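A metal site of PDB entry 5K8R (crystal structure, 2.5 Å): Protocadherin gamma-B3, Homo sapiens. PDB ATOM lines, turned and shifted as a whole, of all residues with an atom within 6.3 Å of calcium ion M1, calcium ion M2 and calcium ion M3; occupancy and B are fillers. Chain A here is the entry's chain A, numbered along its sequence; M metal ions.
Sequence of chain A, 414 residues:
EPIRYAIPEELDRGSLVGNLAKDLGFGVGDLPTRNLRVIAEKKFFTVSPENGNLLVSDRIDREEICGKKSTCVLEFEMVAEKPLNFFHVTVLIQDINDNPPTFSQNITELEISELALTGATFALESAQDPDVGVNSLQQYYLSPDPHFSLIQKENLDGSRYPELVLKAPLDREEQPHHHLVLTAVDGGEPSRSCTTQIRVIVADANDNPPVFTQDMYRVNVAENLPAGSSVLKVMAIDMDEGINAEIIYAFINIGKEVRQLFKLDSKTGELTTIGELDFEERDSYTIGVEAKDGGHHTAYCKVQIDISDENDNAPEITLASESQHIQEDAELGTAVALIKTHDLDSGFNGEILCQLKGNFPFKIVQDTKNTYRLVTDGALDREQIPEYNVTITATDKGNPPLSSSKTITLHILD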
ATOM      1  N   GLU A   9       9.837 -27.288   9.211  1.00  0.00           N
ATOM      2  CA  GLU A   9       9.702 -28.731   9.207  1.00  0.00           C
ATOM      3  C   GLU A   9       8.452 -29.160   9.963  1.00  0.00           C
ATOM      4  O   GLU A   9       7.791 -28.365  10.649  1.00  0.00           O
ATOM      5  CB  GLU A   9      10.941 -29.389   9.826  1.00  0.00           C
ATOM      6  CG  GLU A   9      11.256 -28.871  11.224  1.00  0.00           C
ATOM      7  CD  GLU A   9      12.280 -29.730  11.952  1.00  0.00           C
ATOM      8  OE1 GLU A   9      12.354 -30.945  11.676  1.00  0.00           O
ATOM      9  OE2 GLU A   9      13.015 -29.185  12.798  1.00  0.00           O
ATOM     10  N   GLU A  10       8.108 -30.439   9.824  1.00  0.00           N
ATOM     11  CA  GLU A  10       7.025 -31.076  10.574  1.00  0.00           C
ATOM     12  C   GLU A  10       5.665 -30.446  10.304  1.00  0.00           C
ATOM     13  O   GLU A  10       4.796 -30.407  11.177  1.00  0.00           O
ATOM     14  CB  GLU A  10       7.321 -31.065  12.087  1.00  0.00           C
ATOM     15  CG  GLU A  10       8.670 -31.649  12.466  1.00  0.00           C
ATOM     16  CD  GLU A  10       8.712 -33.164  12.364  1.00  0.00           C
ATOM     17  OE1 GLU A  10       7.649 -33.779  12.125  1.00  0.00           O
ATOM     18  OE2 GLU A  10       9.807 -33.739  12.530  1.00  0.00           O
ATOM     19  N   ARG A  59       5.722 -36.551   6.014  1.00  0.00           N
ATOM     20  CA  ARG A  59       6.403 -35.895   7.110  1.00  0.00           C
ATOM     21  C   ARG A  59       7.802 -35.470   6.697  1.00  0.00           C
ATOM     22  O   ARG A  59       8.585 -36.277   6.168  1.00  0.00           O
ATOM     23  CB  ARG A  59       6.476 -36.827   8.328  1.00  0.00           C
ATOM     24  CG  ARG A  59       7.269 -36.257   9.484  1.00  0.00           C
ATOM     25  CD  ARG A  59       7.107 -37.099  10.734  1.00  0.00           C
ATOM     26  NE  ARG A  59       7.850 -36.550  11.867  1.00  0.00           N
ATOM     27  CZ  ARG A  59       9.049 -36.982  12.263  1.00  0.00           C
ATOM     28  NH1 ARG A  59       9.638 -37.979  11.625  1.00  0.00           N
ATOM     29  NH2 ARG A  59       9.649 -36.416  13.295  1.00  0.00           N
ATOM     30  N   ILE A  60       8.130 -34.204   6.926  1.00  0.00           N
ATOM     31  CA  ILE A  60       9.444 -33.671   6.619  1.00  0.00           C
ATOM     32  C   ILE A  60      10.185 -33.394   7.919  1.00  0.00           C
ATOM     33  O   ILE A  60      10.038 -32.311   8.510  1.00  0.00           O
ATOM     34  CB  ILE A  60       9.352 -32.402   5.741  1.00  0.00           C
ATOM     35  CG1 ILE A  60       8.590 -32.709   4.451  1.00  0.00           C
ATOM     36  CG2 ILE A  60      10.739 -31.858   5.422  1.00  0.00           C
ATOM     37  CD1 ILE A  60       8.455 -31.528   3.525  1.00  0.00           C
ATOM     38  N   ASP A  61      10.958 -34.360   8.392  1.00  0.00           N
ATOM     39  CA  ASP A  61      11.732 -34.228   9.615  1.00  0.00           C
ATOM     40  C   ASP A  61      13.137 -33.763   9.263  1.00  0.00           C
ATOM     41  O   ASP A  61      13.911 -34.514   8.648  1.00  0.00           O
ATOM     42  CB  ASP A  61      11.761 -35.551  10.374  1.00  0.00           C
ATOM     43  CG  ASP A  61      12.659 -35.509  11.596  1.00  0.00           C
ATOM     44  OD1 ASP A  61      12.820 -34.419  12.184  1.00  0.00           O
ATOM     45  OD2 ASP A  61      13.207 -36.571  11.977  1.00  0.00           O
ATOM     46  N   ARG A  62      13.474 -32.533   9.644  1.00  0.00           N
ATOM     47  CA  ARG A  62      14.783 -31.984   9.304  1.00  0.00           C
ATOM     48  C   ARG A  62      15.914 -32.748   9.977  1.00  0.00           C
ATOM     49  O   ARG A  62      17.019 -32.841   9.424  1.00  0.00           O
ATOM     50  CB  ARG A  62      14.848 -30.508   9.674  1.00  0.00           C
ATOM     51  CG  ARG A  62      16.060 -29.777   9.117  1.00  0.00           C
ATOM     52  CD  ARG A  62      16.552 -28.713  10.078  1.00  0.00           C
ATOM     53  NE  ARG A  62      16.936 -29.282  11.363  1.00  0.00           N
ATOM     54  CZ  ARG A  62      18.115 -29.849  11.597  1.00  0.00           C
ATOM     55  NH1 ARG A  62      19.032 -29.922  10.643  1.00  0.00           N
ATOM     56  NH2 ARG A  62      18.382 -30.356  12.797  1.00  0.00           N
ATOM     57  N   GLU A  63      15.669 -33.293  11.179  1.00  0.00           N
ATOM     58  CA  GLU A  63      16.708 -34.046  11.869  1.00  0.00           C
ATOM     59  C   GLU A  63      17.077 -35.319  11.112  1.00  0.00           C
ATOM     60  O   GLU A  63      18.255 -35.684  11.040  1.00  0.00           O
ATOM     61  CB  GLU A  63      16.256 -34.381  13.290  1.00  0.00           C
ATOM     62  CG  GLU A  63      16.469 -33.263  14.293  1.00  0.00           C
ATOM     63  CD  GLU A  63      15.551 -32.078  14.054  1.00  0.00           C
ATOM     64  OE1 GLU A  63      14.340 -32.288  13.849  1.00  0.00           O
ATOM     65  OE2 GLU A  63      16.050 -30.934  14.059  1.00  0.00           O
ATOM     66  N   GLU A  64      16.089 -35.994  10.539  1.00  0.00           N
ATOM     67  CA  GLU A  64      16.362 -37.225   9.801  1.00  0.00           C
ATOM     68  C   GLU A  64      16.902 -36.947   8.401  1.00  0.00           C
ATOM     69  O   GLU A  64      17.637 -37.764   7.851  1.00  0.00           O
ATOM     70  CB  GLU A  64      15.097 -38.083   9.726  1.00  0.00           C
ATOM     71  CG  GLU A  64      15.323 -39.478   9.159  1.00  0.00           C
ATOM     72  CD  GLU A  64      14.046 -40.291   9.138  1.00  0.00           C
ATOM     73  OE1 GLU A  64      12.972 -39.737   9.467  1.00  0.00           O
ATOM     74  OE2 GLU A  64      14.113 -41.491   8.774  1.00  0.00           O
ATOM     75  N   ASP A  95      14.423 -25.147  10.707  1.00  0.00           N
ATOM     76  CA  ASP A  95      14.477 -25.973  11.918  1.00  0.00           C
ATOM     77  C   ASP A  95      13.565 -25.397  12.990  1.00  0.00           C
ATOM     78  O   ASP A  95      13.532 -24.181  13.217  1.00  0.00           O
ATOM     79  CB  ASP A  95      15.919 -26.052  12.440  1.00  0.00           C
ATOM     80  CG  ASP A  95      16.027 -26.912  13.691  1.00  0.00           C
ATOM     81  OD1 ASP A  95      15.447 -28.028  13.710  1.00  0.00           O
ATOM     82  OD2 ASP A  95      16.694 -26.477  14.650  1.00  0.00           O
ATOM     83  N   ILE A  96      12.831 -26.288  13.663  1.00  0.00           N
ATOM     84  CA  ILE A  96      12.035 -25.928  14.826  1.00  0.00           C
ATOM     85  C   ILE A  96      12.603 -26.664  16.030  1.00  0.00           C
ATOM     86  O   ILE A  96      13.253 -27.702  15.912  1.00  0.00           O
ATOM     87  CB  ILE A  96      10.536 -26.242  14.633  1.00  0.00           C
ATOM     88  CG1 ILE A  96      10.322 -27.757  14.513  1.00  0.00           C
ATOM     89  CG2 ILE A  96       9.992 -25.518  13.417  1.00  0.00           C
ATOM     90  CD1 ILE A  96       8.862 -28.147  14.317  1.00  0.00           C
ATOM     91  N   ASN A  97      12.342 -26.110  17.216  1.00  0.00           N
ATOM     92  CA  ASN A  97      12.849 -26.681  18.465  1.00  0.00           C
ATOM     93  C   ASN A  97      11.856 -27.730  18.961  1.00  0.00           C
ATOM     94  O   ASN A  97      11.099 -27.517  19.919  1.00  0.00           O
ATOM     95  CB  ASN A  97      13.084 -25.592  19.507  1.00  0.00           C
ATOM     96  CG  ASN A  97      13.809 -26.109  20.732  1.00  0.00           C
ATOM     97  OD1 ASN A  97      14.644 -27.004  20.639  1.00  0.00           O
ATOM     98  ND2 ASN A  97      13.481 -25.561  21.890  1.00  0.00           N
ATOM     99  N   ASP A  98      11.853 -28.883  18.301  1.00  0.00           N
ATOM    100  CA  ASP A  98      10.980 -29.989  18.657  1.00  0.00           C
ATOM    101  C   ASP A  98      11.740 -31.161  19.277  1.00  0.00           C
ATOM    102  O   ASP A  98      11.185 -32.253  19.384  1.00  0.00           O
ATOM    103  CB  ASP A  98      10.193 -30.455  17.428  1.00  0.00           C
ATOM    104  CG  ASP A  98      11.088 -30.874  16.288  1.00  0.00           C
ATOM    105  OD1 ASP A  98      12.256 -30.434  16.249  1.00  0.00           O
ATOM    106  OD2 ASP A  98      10.620 -31.649  15.421  1.00  0.00           O
ATOM    107  N   ASN A  99      12.983 -30.946  19.680  1.00  0.00           N
ATOM    108  CA  ASN A  99      13.793 -31.982  20.302  1.00  0.00           C
ATOM    109  C   ASN A  99      14.432 -31.418  21.567  1.00  0.00           C
ATOM    110  O   ASN A  99      15.057 -30.346  21.519  1.00  0.00           O
ATOM    111  CB  ASN A  99      14.877 -32.500  19.350  1.00  0.00           C
ATOM    112  CG  ASN A  99      14.316 -33.378  18.249  1.00  0.00           C
ATOM    113  OD1 ASN A  99      14.380 -33.025  17.072  1.00  0.00           O
ATOM    114  ND2 ASN A  99      13.762 -34.525  18.634  1.00  0.00           N
ATOM    115  N   PRO A 100      14.304 -32.094  22.707  1.00  0.00           N
ATOM    116  CA  PRO A 100      14.945 -31.624  23.919  1.00  0.00           C
ATOM    117  C   PRO A 100      16.401 -32.059  23.966  1.00  0.00           C
ATOM    118  O   PRO A 100      16.792 -33.007  23.272  1.00  0.00           O
ATOM    119  CB  PRO A 100      14.129 -32.306  25.025  1.00  0.00           C
ATOM    120  CG  PRO A 100      13.717 -33.601  24.411  1.00  0.00           C
ATOM    121  CD  PRO A 100      13.489 -33.302  22.945  1.00  0.00           C
ATOM    122  N   PRO A 101      17.233 -31.387  24.767  1.00  0.00           N
ATOM    123  CA  PRO A 101      18.588 -31.885  24.982  1.00  0.00           C
ATOM    124  C   PRO A 101      18.560 -33.192  25.753  1.00  0.00           C
ATOM    125  O   PRO A 101      17.548 -33.588  26.339  1.00  0.00           O
ATOM    126  CB  PRO A 101      19.250 -30.774  25.812  1.00  0.00           C
ATOM    127  CG  PRO A 101      18.104 -30.057  26.465  1.00  0.00           C
ATOM    128  CD  PRO A 101      16.976 -30.124  25.482  1.00  0.00           C
ATOM    129  N   ASP A 129      21.897 -32.413  21.363  1.00  0.00           N
ATOM    130  CA  ASP A 129      20.627 -31.920  20.845  1.00  0.00           C
ATOM    131  C   ASP A 129      20.611 -32.073  19.324  1.00  0.00           C
ATOM    132  O   ASP A 129      21.428 -31.457  18.625  1.00  0.00           O
ATOM    133  CB  ASP A 129      20.416 -30.459  21.240  1.00  0.00           C
ATOM    134  CG  ASP A 129      18.969 -30.027  21.143  1.00  0.00           C
ATOM    135  OD1 ASP A 129      18.327 -30.321  20.110  1.00  0.00           O
ATOM    136  OD2 ASP A 129      18.480 -29.382  22.092  1.00  0.00           O
ATOM    137  N   PRO A 130      19.697 -32.885  18.768  1.00  0.00           N
ATOM    138  CA  PRO A 130      19.685 -33.091  17.319  1.00  0.00           C
ATOM    139  C   PRO A 130      19.243 -31.886  16.519  1.00  0.00           C
ATOM    140  O   PRO A 130      19.328 -31.915  15.280  1.00  0.00           O
ATOM    141  CB  PRO A 130      18.711 -34.271  17.137  1.00  0.00           C
ATOM    142  CG  PRO A 130      17.823 -34.189  18.332  1.00  0.00           C
ATOM    143  CD  PRO A 130      18.668 -33.684  19.459  1.00  0.00           C
ATOM    144  N   ASP A 131      18.759 -30.825  17.175  1.00  0.00           N
ATOM    145  CA  ASP A 131      18.404 -29.606  16.466  1.00  0.00           C
ATOM    146  C   ASP A 131      19.676 -28.865  16.043  1.00  0.00           C
ATOM    147  O   ASP A 131      20.801 -29.303  16.290  1.00  0.00           O
ATOM    148  CB  ASP A 131      17.524 -28.718  17.343  1.00  0.00           C
ATOM    149  CG  ASP A 131      16.187 -29.373  17.671  1.00  0.00           C
ATOM    150  OD1 ASP A 131      15.686 -30.148  16.834  1.00  0.00           O
ATOM    151  OD2 ASP A 131      15.649 -29.102  18.770  1.00  0.00           O
ATOM    152  N   VAL A 132      19.493 -27.720  15.387  1.00  0.00           N
ATOM    153  CA  VAL A 132      20.593 -26.885  14.924  1.00  0.00           C
ATOM    154  C   VAL A 132      20.317 -25.439  15.281  1.00  0.00           C
ATOM    155  O   VAL A 132      19.202 -25.077  15.694  1.00  0.00           O
ATOM    156  CB  VAL A 132      20.830 -27.034  13.400  1.00  0.00           C
ATOM    157  CG1 VAL A 132      21.390 -28.415  13.080  1.00  0.00           C
ATOM    158  CG2 VAL A 132      19.552 -26.777  12.638  1.00  0.00           C
ATOM    159  N   VAL A 134      20.130 -22.003  17.252  1.00  0.00           N
ATOM    160  CA  VAL A 134      19.844 -21.726  18.661  1.00  0.00           C
ATOM    161  C   VAL A 134      19.017 -22.822  19.297  1.00  0.00           C
ATOM    162  O   VAL A 134      18.990 -22.935  20.535  1.00  0.00           O
ATOM    163  CB  VAL A 134      19.134 -20.365  18.797  1.00  0.00           C
ATOM    164  CG1 VAL A 134      20.032 -19.241  18.302  1.00  0.00           C
ATOM    165  CG2 VAL A 134      17.818 -20.371  18.048  1.00  0.00           C
ATOM    166  N   ASN A 135      18.340 -23.649  18.490  1.00  0.00           N
ATOM    167  CA  ASN A 135      17.526 -24.724  19.046  1.00  0.00           C
ATOM    168  C   ASN A 135      18.370 -25.819  19.687  1.00  0.00           C
ATOM    169  O   ASN A 135      17.845 -26.614  20.466  1.00  0.00           O
ATOM    170  CB  ASN A 135      16.636 -25.320  17.957  1.00  0.00           C
ATOM    171  CG  ASN A 135      15.710 -24.309  17.339  1.00  0.00           C
ATOM    172  OD1 ASN A 135      15.356 -23.304  17.968  1.00  0.00           O
ATOM    173  ND2 ASN A 135      15.304 -24.552  16.094  1.00  0.00           N
ATOM    174  N   SER A 136      19.672 -25.868  19.382  1.00  0.00           N
ATOM    175  CA  SER A 136      20.582 -26.809  20.022  1.00  0.00           C
ATOM    176  C   SER A 136      21.632 -26.120  20.893  1.00  0.00           C
ATOM    177  O   SER A 136      22.391 -26.820  21.571  1.00  0.00           O
ATOM    178  CB  SER A 136      21.291 -27.677  18.978  1.00  0.00           C
ATOM    179  OG  SER A 136      22.047 -26.877  18.088  1.00  0.00           O
ATOM    180  N   GLN A 138      23.042 -24.848  24.002  1.00  0.00           N
ATOM    181  CA  GLN A 138      22.685 -25.246  25.347  1.00  0.00           C
ATOM    182  C   GLN A 138      23.145 -24.232  26.387  1.00  0.00           C
ATOM    183  O   GLN A 138      24.090 -23.465  26.169  1.00  0.00           O
ATOM    184  CB  GLN A 138      23.273 -26.623  25.680  1.00  0.00           C
ATOM    185  CG  GLN A 138      22.816 -27.728  24.751  1.00  0.00           C
ATOM    186  CD  GLN A 138      21.303 -27.856  24.690  1.00  0.00           C
ATOM    187  OE1 GLN A 138      20.613 -27.692  25.704  1.00  0.00           O
ATOM    188  NE2 GLN A 138      20.783 -28.122  23.504  1.00  0.00           N
ATOM    189  N   ASP A 186      17.941 -25.565  26.227  1.00  0.00           N
ATOM    190  CA  ASP A 186      18.298 -25.059  24.915  1.00  0.00           C
ATOM    191  C   ASP A 186      17.764 -23.640  24.716  1.00  0.00           C
ATOM    192  O   ASP A 186      17.063 -23.091  25.569  1.00  0.00           O
ATOM    193  CB  ASP A 186      17.787 -26.006  23.816  1.00  0.00           C
ATOM    194  CG  ASP A 186      16.301 -26.286  23.914  1.00  0.00           C
ATOM    195  OD1 ASP A 186      15.537 -25.427  24.424  1.00  0.00           O
ATOM    196  OD2 ASP A 186      15.877 -27.370  23.468  1.00  0.00           O
ATOM    197  N   GLY A 187      18.104 -23.037  23.581  1.00  0.00           N
ATOM    198  CA  GLY A 187      17.696 -21.676  23.309  1.00  0.00           C
ATOM    199  C   GLY A 187      16.612 -21.564  22.254  1.00  0.00           C
ATOM    200  O   GLY A 187      16.494 -20.540  21.591  1.00  0.00           O
ATOM    201  N   GLY A 188      15.822 -22.628  22.083  1.00  0.00           N
ATOM    202  CA  GLY A 188      14.769 -22.645  21.104  1.00  0.00           C
ATOM    203  C   GLY A 188      13.436 -22.194  21.675  1.00  0.00           C
ATOM    204  O   GLY A 188      13.311 -21.787  22.826  1.00  0.00           O
ATOM    205  N   ARG A 192      13.358 -26.151  25.886  1.00  0.00           N
ATOM    206  CA  ARG A 192      13.359 -27.550  26.312  1.00  0.00           C
ATOM    207  C   ARG A 192      14.613 -27.822  27.128  1.00  0.00           C
ATOM    208  O   ARG A 192      15.683 -27.268  26.842  1.00  0.00           O
ATOM    209  CB  ARG A 192      13.296 -28.493  25.105  1.00  0.00           C
ATOM    210  CG  ARG A 192      11.940 -28.491  24.405  1.00  0.00           C
ATOM    211  CD  ARG A 192      11.949 -29.390  23.178  1.00  0.00           C
ATOM    212  NE  ARG A 192      10.662 -30.051  22.984  1.00  0.00           N
ATOM    213  CZ  ARG A 192       9.618 -29.494  22.370  1.00  0.00           C
ATOM    214  NH1 ARG A 192       9.712 -28.265  21.891  1.00  0.00           N
ATOM    215  NH2 ARG A 192       8.488 -30.178  22.238  1.00  0.00           N
HETATM  216 CA    CA M   1      14.189 -29.676  14.928  1.00  0.00          CA
HETATM  217 CA    CA M   2      16.504 -28.519  21.060  1.00  0.00          CA
HETATM  218 CA    CA M   3      11.943 -32.729  13.675  1.00  0.00          CA
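OE1 of Glu 9 lies close to N of Arg 62 (2.8 Å).
OE1 of Glu 10 is in salt-bridge range of NE of Arg 59, at 2.8 Å.
The backbone NH of Val 132 sits at hydrogen-bond distance from the side-chain carboxylate of Asp 95 (3.2 Å).
N of Glu 64 is in hydrogen-bond range of OD2 of Asp 61 (3.3 Å).
The side-chain carboxylate (OD2) of Asp 61 lies within salt-bridge range of the guanidinium group (NH2) of Arg 59.
The side-chain carboxylate of Glu 63 lies close to the side-chain amide oxygen of Asn 99, at 3.3 Å.
OD1 of Asp 186 sits at hydrogen-bond distance from N of Arg 192.
O of Asn 97 lies within hydrogen-bond range of NH1 of Arg 192, 2.5 Å away.
Along chain A the residues within 4 Å of calcium ion M1 span positions 9 to 131.
Within 4 Å of calcium ion M2: Asn 97, Asn 99, Asp 129, Asp 131, Asn 135 and Asp 186.
The nearest printed residue that does not touch calcium ion M2 is Ser 136 (4.5 Å).
Five residues have an atom within 4 Å of calcium ion M3: Glu 9, Glu 10, Asp 61, Glu 63 and Asp 98.
The backbone carbonyl oxygen (O) of Ile 96 is bound to calcium ion M1 (2.4 Å).
OD1 of Asp 95 is bound to calcium ion M1, 2.4 Å away.
Calcium ion M1 is bound by OE2 of Glu 63 (2.4 Å).
The side-chain carboxylate (OD1) of Asp 98 binds calcium ion M1.
Calcium ion M1 is bound by the side-chain carboxylate (OD1) of Asp 131, 2.5 Å away.
The side-chain carboxylate (OE2) of Glu 9 is bound to calcium ion M1, 2.5 Å away.
OE1 of Glu 63 binds calcium ion M1 (2.8 Å).
Calcium ion M1 has seven donor atoms within binding distance.
Calcium ion M2 is bound by the backbone carbonyl oxygen (O) of Asn 99 (2.4 Å).
Calcium ion M2 is bound by the side-chain carboxylate (OD2) of Asp 129, 2.4 Å away.
The backbone carbonyl oxygen (O) of Asn 135 is bound to calcium ion M2, 2.4 Å away.
OD1 of Asn 97 binds calcium ion M2 (2.4 Å).
The side-chain carboxylate (OD2) of Asp 131 binds calcium ion M2, at 2.5 Å.
Calcium ion M2 is bound by OD1 of Asp 129 (2.7 Å).
Calcium ion M2 is bound by OD2 of Asp 186.
Calcium ion M3 is bound by OD1 of Asp 61 (2.4 Å).
Calcium ion M3 is bound by OD2 of Asp 98, 2.4 Å away.
Calcium ion M3 is bound by the side-chain carboxylate (OE1) of Glu 63, at 2.4 Å.
OE2 of Glu 10 is bound to calcium ion M3, 2.6 Å away.
OE1 of Glu 9 is bound to calcium ion M3, 2.7 Å away.
Calcium ion M3 has five donor atoms within binding distance.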
